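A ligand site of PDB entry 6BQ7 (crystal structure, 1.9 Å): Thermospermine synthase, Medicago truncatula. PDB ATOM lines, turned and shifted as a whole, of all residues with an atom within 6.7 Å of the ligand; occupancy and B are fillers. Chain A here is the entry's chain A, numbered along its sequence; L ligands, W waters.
N of Leu 77 sits at hydrogen-bond distance from OH of Tyr 31 (3.5 Å). The backbone carbonyl oxygen of Leu 182 lies within hydrogen-bond range of the side-chain amide nitrogen of Gln 217. The side-chain carboxylate (OE1) of Glu 33 is in hydrogen-bond range of the backbone NH (N) of Leu 77, at 3.1 Å. The side-chain carboxylate (OE1) of Glu 33 lies within hydrogen-bond range of the side-chain hydroxyl (OH) of Tyr 31 (2.9 Å). OH of Tyr 254 lies within hydrogen-bond range of O of Gln 78. NE2 of Gln 78 sits close to O of Lys 76 (3.5 Å). N of Trp 41 is in hydrogen-bond range of O of Glu 33. The side-chain hydroxyl (OH) of Tyr 87 lies within hydrogen-bond range of the side-chain carboxylate (OD1) of Asp 181, at 2.7 Å.
Water W2 bridges the side-chain amino group (NZ) of Lys 76 and a nitrogen (N2) of the ligand.
Lys 76 touches the ligand. OH of Tyr 87 touches C6 of the ligand, at 3.8 Å. Leu 182 touches the ligand (O to C6, 3.7 Å). Tyr 254 touches the ligand. Trp 258 touches the ligand (CH2 to C3, 3.6 Å). Of the 22 residues printed, 9 come within 4 Å of the ligand.
The side-chain amide oxygen (OE1) of Gln 78 lies within hydrogen-bond range of a nitrogen (N2) of the ligand. A nitrogen (N3) of the ligand is in salt-bridge range of the side-chain carboxylate (OD1) of Asp 181, 3.1 Å away. The backbone carbonyl oxygen (O) of Asp 181 lies within hydrogen-bond range of a nitrogen (N3) of the ligand (3.4 Å). The side-chain carboxylate (OE2) of Glu 33 lies within salt-bridge range of a nitrogen (N1) of the ligand, at 3.0 Å. A nitrogen (N1) of the ligand lies close to the backbone carbonyl oxygen (O) of Leu 77 (3.4 Å).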
ATOM      1  N   TYR A  31      18.953  25.524  13.324  1.00  0.00           N
ATOM      2  CA  TYR A  31      19.977  25.519  12.309  1.00  0.00           C
ATOM      3  C   TYR A  31      19.413  24.793  11.094  1.00  0.00           C
ATOM      4  O   TYR A  31      18.840  23.702  11.225  1.00  0.00           O
ATOM      5  CB  TYR A  31      21.254  24.839  12.802  1.00  0.00           C
ATOM      6  CG  TYR A  31      22.153  24.395  11.673  1.00  0.00           C
ATOM      7  CD1 TYR A  31      22.842  25.307  10.902  1.00  0.00           C
ATOM      8  CD2 TYR A  31      22.270  23.037  11.353  1.00  0.00           C
ATOM      9  CE1 TYR A  31      23.648  24.905   9.867  1.00  0.00           C
ATOM     10  CE2 TYR A  31      23.081  22.617  10.316  1.00  0.00           C
ATOM     11  CZ  TYR A  31      23.765  23.553   9.578  1.00  0.00           C
ATOM     12  OH  TYR A  31      24.577  23.165   8.535  1.00  0.00           O
ATOM     13  N   GLU A  33      19.979  23.478   7.053  1.00  0.00           N
ATOM     14  CA  GLU A  33      20.922  23.144   6.038  1.00  0.00           C
ATOM     15  C   GLU A  33      20.219  22.610   4.829  1.00  0.00           C
ATOM     16  O   GLU A  33      19.385  21.765   4.922  1.00  0.00           O
ATOM     17  CB  GLU A  33      21.925  22.117   6.501  1.00  0.00           C
ATOM     18  CG  GLU A  33      23.032  21.935   5.486  1.00  0.00           C
ATOM     19  CD  GLU A  33      24.121  21.001   5.916  1.00  0.00           C
ATOM     20  OE1 GLU A  33      24.199  20.678   7.080  1.00  0.00           O
ATOM     21  OE2 GLU A  33      24.897  20.579   5.083  1.00  0.00           O
ATOM     22  N   ILE A  35      20.419  20.311   2.256  1.00  0.00           N
ATOM     23  CA  ILE A  35      21.116  19.136   1.839  1.00  0.00           C
ATOM     24  C   ILE A  35      21.184  19.070   0.337  1.00  0.00           C
ATOM     25  O   ILE A  35      22.188  18.786  -0.220  1.00  0.00           O
ATOM     26  CB  ILE A  35      20.377  17.886   2.202  1.00  0.00           C
ATOM     27  CG1 ILE A  35      20.269  17.732   3.687  1.00  0.00           C
ATOM     28  CG2 ILE A  35      21.144  16.742   1.653  1.00  0.00           C
ATOM     29  CD1 ILE A  35      21.547  18.069   4.402  1.00  0.00           C
ATOM     30  N   TRP A  41      17.072  20.343   6.021  1.00  0.00           N
ATOM     31  CA  TRP A  41      17.273  19.532   7.229  1.00  0.00           C
ATOM     32  C   TRP A  41      17.547  20.521   8.320  1.00  0.00           C
ATOM     33  O   TRP A  41      18.470  21.243   8.234  1.00  0.00           O
ATOM     34  CB  TRP A  41      18.494  18.712   6.926  1.00  0.00           C
ATOM     35  CG  TRP A  41      18.921  17.665   7.782  1.00  0.00           C
ATOM     36  CD1 TRP A  41      20.172  17.451   8.149  1.00  0.00           C
ATOM     37  CD2 TRP A  41      18.164  16.603   8.314  1.00  0.00           C
ATOM     38  NE1 TRP A  41      20.258  16.344   8.898  1.00  0.00           N
ATOM     39  CE2 TRP A  41      19.033  15.805   9.011  1.00  0.00           C
ATOM     40  CE3 TRP A  41      16.836  16.256   8.289  1.00  0.00           C
ATOM     41  CZ2 TRP A  41      18.634  14.709   9.676  1.00  0.00           C
ATOM     42  CZ3 TRP A  41      16.453  15.176   8.954  1.00  0.00           C
ATOM     43  CH2 TRP A  41      17.334  14.413   9.645  1.00  0.00           C
ATOM     44  N   LEU A  73      31.172  24.119   8.332  1.00  0.00           N
ATOM     45  CA  LEU A  73      32.164  24.849   7.533  1.00  0.00           C
ATOM     46  C   LEU A  73      31.483  25.299   6.258  1.00  0.00           C
ATOM     47  O   LEU A  73      30.878  24.481   5.549  1.00  0.00           O
ATOM     48  CB  LEU A  73      33.390  23.978   7.223  1.00  0.00           C
ATOM     49  CG  LEU A  73      34.082  23.379   8.456  1.00  0.00           C
ATOM     50  CD1 LEU A  73      35.236  22.492   8.048  1.00  0.00           C
ATOM     51  CD2 LEU A  73      34.563  24.468   9.425  1.00  0.00           C
ATOM     52  N   LYS A  76      27.972  24.095   5.691  1.00  0.00           N
ATOM     53  CA  LYS A  76      27.724  22.652   5.577  1.00  0.00           C
ATOM     54  C   LYS A  76      28.172  21.966   6.846  1.00  0.00           C
ATOM     55  O   LYS A  76      29.352  22.067   7.222  1.00  0.00           O
ATOM     56  CB  LYS A  76      28.473  22.071   4.370  1.00  0.00           C
ATOM     57  CG  LYS A  76      28.142  22.746   3.050  1.00  0.00           C
ATOM     58  CD  LYS A  76      29.045  22.251   1.915  1.00  0.00           C
ATOM     59  CE  LYS A  76      28.649  20.853   1.453  1.00  0.00           C
ATOM     60  NZ  LYS A  76      29.490  19.786   2.064  1.00  0.00           N
ATOM     61  N   LEU A  77      27.255  21.249   7.499  1.00  0.00           N
ATOM     62  CA  LEU A  77      27.650  20.442   8.644  1.00  0.00           C
ATOM     63  C   LEU A  77      28.703  19.438   8.195  1.00  0.00           C
ATOM     64  O   LEU A  77      28.514  18.733   7.199  1.00  0.00           O
ATOM     65  CB  LEU A  77      26.443  19.714   9.245  1.00  0.00           C
ATOM     66  CG  LEU A  77      26.733  19.005  10.572  1.00  0.00           C
ATOM     67  CD1 LEU A  77      25.539  19.115  11.482  1.00  0.00           C
ATOM     68  CD2 LEU A  77      27.074  17.535  10.373  1.00  0.00           C
ATOM     69  N   GLN A  78      29.826  19.415   8.912  1.00  0.00           N
ATOM     70  CA  GLN A  78      30.893  18.483   8.635  1.00  0.00           C
ATOM     71  C   GLN A  78      31.045  17.435   9.722  1.00  0.00           C
ATOM     72  O   GLN A  78      31.618  16.379   9.463  1.00  0.00           O
ATOM     73  CB  GLN A  78      32.224  19.222   8.451  1.00  0.00           C
ATOM     74  CG  GLN A  78      32.227  20.231   7.287  1.00  0.00           C
ATOM     75  CD  GLN A  78      31.998  19.594   5.928  1.00  0.00           C
ATOM     76  OE1 GLN A  78      32.363  18.430   5.699  1.00  0.00           O
ATOM     77  NE2 GLN A  78      31.399  20.335   5.022  1.00  0.00           N
ATOM     78  N   SER A  79      30.526  17.694  10.919  1.00  0.00           N
ATOM     79  CA  SER A  79      30.816  16.856  12.067  1.00  0.00           C
ATOM     80  C   SER A  79      29.818  17.172  13.164  1.00  0.00           C
ATOM     81  O   SER A  79      29.674  18.344  13.540  1.00  0.00           O
ATOM     82  CB  SER A  79      32.238  17.104  12.547  1.00  0.00           C
ATOM     83  OG  SER A  79      32.692  16.026  13.325  1.00  0.00           O
ATOM     84  N   TYR A  87      31.479   8.355  10.919  1.00  0.00           N
ATOM     85  CA  TYR A  87      32.226   8.818   9.767  1.00  0.00           C
ATOM     86  C   TYR A  87      33.699   8.541   9.937  1.00  0.00           C
ATOM     87  O   TYR A  87      34.344   8.023   9.009  1.00  0.00           O
ATOM     88  CB  TYR A  87      31.988  10.320   9.559  1.00  0.00           C
ATOM     89  CG  TYR A  87      32.867  10.875   8.471  1.00  0.00           C
ATOM     90  CD1 TYR A  87      32.475  10.796   7.142  1.00  0.00           C
ATOM     91  CD2 TYR A  87      34.099  11.433   8.776  1.00  0.00           C
ATOM     92  CE1 TYR A  87      33.304  11.280   6.138  1.00  0.00           C
ATOM     93  CE2 TYR A  87      34.929  11.915   7.792  1.00  0.00           C
ATOM     94  CZ  TYR A  87      34.525  11.842   6.474  1.00  0.00           C
ATOM     95  OH  TYR A  87      35.356  12.356   5.485  1.00  0.00           O
ATOM     96  N   HIS A  88      34.246   8.887  11.061  1.00  0.00           N
ATOM     97  CA  HIS A  88      35.662   8.707  11.309  1.00  0.00           C
ATOM     98  C   HIS A  88      36.130   7.269  11.469  1.00  0.00           C
ATOM     99  O   HIS A  88      37.198   6.964  11.087  1.00  0.00           O
ATOM    100  CB  HIS A  88      36.143   9.630  12.396  1.00  0.00           C
ATOM    101  CG  HIS A  88      36.005  11.060  12.030  1.00  0.00           C
ATOM    102  ND1 HIS A  88      35.016  11.854  12.525  1.00  0.00           N
ATOM    103  CD2 HIS A  88      36.684  11.819  11.146  1.00  0.00           C
ATOM    104  CE1 HIS A  88      35.109  13.050  11.998  1.00  0.00           C
ATOM    105  NE2 HIS A  88      36.117  13.044  11.156  1.00  0.00           N
ATOM    106  N   GLY A 110      41.649  16.698   7.114  1.00  0.00           N
ATOM    107  CA  GLY A 110      41.564  16.241   8.494  1.00  0.00           C
ATOM    108  C   GLY A 110      41.792  17.281   9.575  1.00  0.00           C
ATOM    109  O   GLY A 110      42.160  16.923  10.693  1.00  0.00           O
ATOM    110  N   GLU A 112      39.956  18.875  11.568  1.00  0.00           N
ATOM    111  CA  GLU A 112      39.138  18.803  12.780  1.00  0.00           C
ATOM    112  C   GLU A 112      39.774  17.956  13.882  1.00  0.00           C
ATOM    113  O   GLU A 112      39.428  18.119  15.063  1.00  0.00           O
ATOM    114  CB  GLU A 112      37.743  18.294  12.393  1.00  0.00           C
ATOM    115  CG  GLU A 112      37.084  17.374  13.404  1.00  0.00           C
ATOM    116  CD  GLU A 112      35.667  17.015  13.030  1.00  0.00           C
ATOM    117  OE1 GLU A 112      35.193  17.491  11.966  1.00  0.00           O
ATOM    118  OE2 GLU A 112      35.027  16.254  13.799  1.00  0.00           O
ATOM    119  N   ASP A 181      40.636  13.159   3.400  1.00  0.00           N
ATOM    120  CA  ASP A 181      39.540  13.706   4.193  1.00  0.00           C
ATOM    121  C   ASP A 181      39.216  15.123   3.766  1.00  0.00           C
ATOM    122  O   ASP A 181      39.129  16.039   4.599  1.00  0.00           O
ATOM    123  CB  ASP A 181      39.870  13.657   5.681  1.00  0.00           C
ATOM    124  CG  ASP A 181      38.640  13.855   6.565  1.00  0.00           C
ATOM    125  OD1 ASP A 181      37.503  13.942   6.020  1.00  0.00           O
ATOM    126  OD2 ASP A 181      38.818  13.907   7.805  1.00  0.00           O
ATOM    127  N   LEU A 182      39.032  15.334   2.453  1.00  0.00           N
ATOM    128  CA  LEU A 182      38.766  16.649   1.917  1.00  0.00           C
ATOM    129  C   LEU A 182      37.284  16.800   1.598  1.00  0.00           C
ATOM    130  O   LEU A 182      36.502  15.851   1.713  1.00  0.00           O
ATOM    131  CB  LEU A 182      39.608  16.882   0.665  1.00  0.00           C
ATOM    132  CG  LEU A 182      41.083  16.563   0.839  1.00  0.00           C
ATOM    133  CD1 LEU A 182      41.639  16.129  -0.506  1.00  0.00           C
ATOM    134  CD2 LEU A 182      41.818  17.779   1.403  1.00  0.00           C
ATOM    135  N   ALA A 183      36.907  18.005   1.156  1.00  0.00           N
ATOM    136  CA  ALA A 183      35.558  18.292   0.684  1.00  0.00           C
ATOM    137  C   ALA A 183      35.288  17.584  -0.641  1.00  0.00           C
ATOM    138  O   ALA A 183      36.197  17.114  -1.328  1.00  0.00           O
ATOM    139  CB  ALA A 183      35.352  19.796   0.525  1.00  0.00           C
ATOM    140  N   ASP A 184      34.002  17.523  -0.993  1.00  0.00           N
ATOM    141  CA  ASP A 184      33.601  16.811  -2.198  1.00  0.00           C
ATOM    142  C   ASP A 184      34.112  17.537  -3.439  1.00  0.00           C
ATOM    143  O   ASP A 184      34.117  18.765  -3.469  1.00  0.00           O
ATOM    144  CB  ASP A 184      32.076  16.675  -2.250  1.00  0.00           C
ATOM    145  CG  ASP A 184      31.509  15.921  -1.061  1.00  0.00           C
ATOM    146  OD1 ASP A 184      32.240  15.083  -0.501  1.00  0.00           O
ATOM    147  OD2 ASP A 184      30.348  16.188  -0.678  1.00  0.00           O
ATOM    148  N   GLN A 217      37.283   9.748   1.511  1.00  0.00           N
ATOM    149  CA  GLN A 217      35.842   9.937   1.549  1.00  0.00           C
ATOM    150  C   GLN A 217      35.365  10.175   0.128  1.00  0.00           C
ATOM    151  O   GLN A 217      36.095  10.691  -0.722  1.00  0.00           O
ATOM    152  CB  GLN A 217      35.471  11.089   2.496  1.00  0.00           C
ATOM    153  CG  GLN A 217      35.741  12.496   1.955  1.00  0.00           C
ATOM    154  CD  GLN A 217      34.525  13.089   1.264  1.00  0.00           C
ATOM    155  OE1 GLN A 217      33.430  12.523   1.313  1.00  0.00           O
ATOM    156  NE2 GLN A 217      34.702  14.233   0.622  1.00  0.00           N
ATOM    157  N   SER A 253      23.320  12.656  10.998  1.00  0.00           N
ATOM    158  CA  SER A 253      23.488  14.101  10.895  1.00  0.00           C
ATOM    159  C   SER A 253      23.713  14.536   9.442  1.00  0.00           C
ATOM    160  O   SER A 253      23.524  15.720   9.136  1.00  0.00           O
ATOM    161  CB  SER A 253      24.659  14.572  11.769  1.00  0.00           C
ATOM    162  OG  SER A 253      25.853  14.033  11.234  1.00  0.00           O
ATOM    163  N   TYR A 254      24.051  13.649   8.555  1.00  0.00           N
ATOM    164  CA  TYR A 254      24.246  14.013   7.165  1.00  0.00           C
ATOM    165  C   TYR A 254      22.995  13.824   6.357  1.00  0.00           C
ATOM    166  O   TYR A 254      22.960  14.151   5.241  1.00  0.00           O
ATOM    167  CB  TYR A 254      25.295  13.142   6.533  1.00  0.00           C
ATOM    168  CG  TYR A 254      26.674  13.389   6.945  1.00  0.00           C
ATOM    169  CD1 TYR A 254      26.954  14.245   7.956  1.00  0.00           C
ATOM    170  CD2 TYR A 254      27.696  12.724   6.365  1.00  0.00           C
ATOM    171  CE1 TYR A 254      28.217  14.459   8.362  1.00  0.00           C
ATOM    172  CE2 TYR A 254      28.981  12.935   6.768  1.00  0.00           C
ATOM    173  CZ  TYR A 254      29.233  13.814   7.775  1.00  0.00           C
ATOM    174  OH  TYR A 254      30.491  14.046   8.194  1.00  0.00           O
ATOM    175  N   ALA A 255      21.990  13.259   6.956  1.00  0.00           N
ATOM    176  CA  ALA A 255      20.765  12.893   6.314  1.00  0.00           C
ATOM    177  C   ALA A 255      20.965  12.148   5.021  1.00  0.00           C
ATOM    178  O   ALA A 255      20.251  12.427   4.099  1.00  0.00           O
ATOM    179  CB  ALA A 255      19.865  14.090   6.100  1.00  0.00           C
ATOM    180  N   TRP A 258      26.736   7.978   3.440  1.00  0.00           N
ATOM    181  CA  TRP A 258      28.009   8.533   2.992  1.00  0.00           C
ATOM    182  C   TRP A 258      28.912   7.430   2.500  1.00  0.00           C
ATOM    183  O   TRP A 258      28.826   6.276   2.972  1.00  0.00           O
ATOM    184  CB  TRP A 258      28.723   9.307   4.112  1.00  0.00           C
ATOM    185  CG  TRP A 258      29.523  10.432   3.525  1.00  0.00           C
ATOM    186  CD1 TRP A 258      30.881  10.473   3.343  1.00  0.00           C
ATOM    187  CD2 TRP A 258      28.996  11.641   2.982  1.00  0.00           C
ATOM    188  NE1 TRP A 258      31.237  11.651   2.744  1.00  0.00           N
ATOM    189  CE2 TRP A 258      30.099  12.382   2.512  1.00  0.00           C
ATOM    190  CE3 TRP A 258      27.710  12.174   2.865  1.00  0.00           C
ATOM    191  CZ2 TRP A 258      29.952  13.644   1.930  1.00  0.00           C
ATOM    192  CZ3 TRP A 258      27.563  13.436   2.283  1.00  0.00           C
ATOM    193  CH2 TRP A 258      28.683  14.158   1.829  1.00  0.00           C
HETATM  194  N1  LIG L   1      26.047  17.764   5.133  1.00  0.00           N
HETATM  195  C1  LIG L   1      26.720  16.835   4.257  1.00  0.00           C
HETATM  196  C2  LIG L   1      27.910  16.267   5.013  1.00  0.00           C
HETATM  197  C3  LIG L   1      29.198  16.675   4.321  1.00  0.00           C
HETATM  198  C4  LIG L   1      30.337  15.836   4.902  1.00  0.00           C
HETATM  199  N2  LIG L   1      31.605  16.175   4.283  1.00  0.00           N
HETATM  200  C5  LIG L   1      32.577  15.132   4.584  1.00  0.00           C
HETATM  201  C6  LIG L   1      33.982  15.690   4.420  1.00  0.00           C
HETATM  202  C7  LIG L   1      34.547  16.075   5.790  1.00  0.00           C
HETATM  203  N3  LIG L   1      35.888  16.603   5.627  1.00  0.00           N
HETATM  204  O   HOH W   1      24.162  15.527   2.828  1.00  0.00           O
HETATM  205  O   HOH W   2      31.889  18.369   1.816  1.00  0.00           O
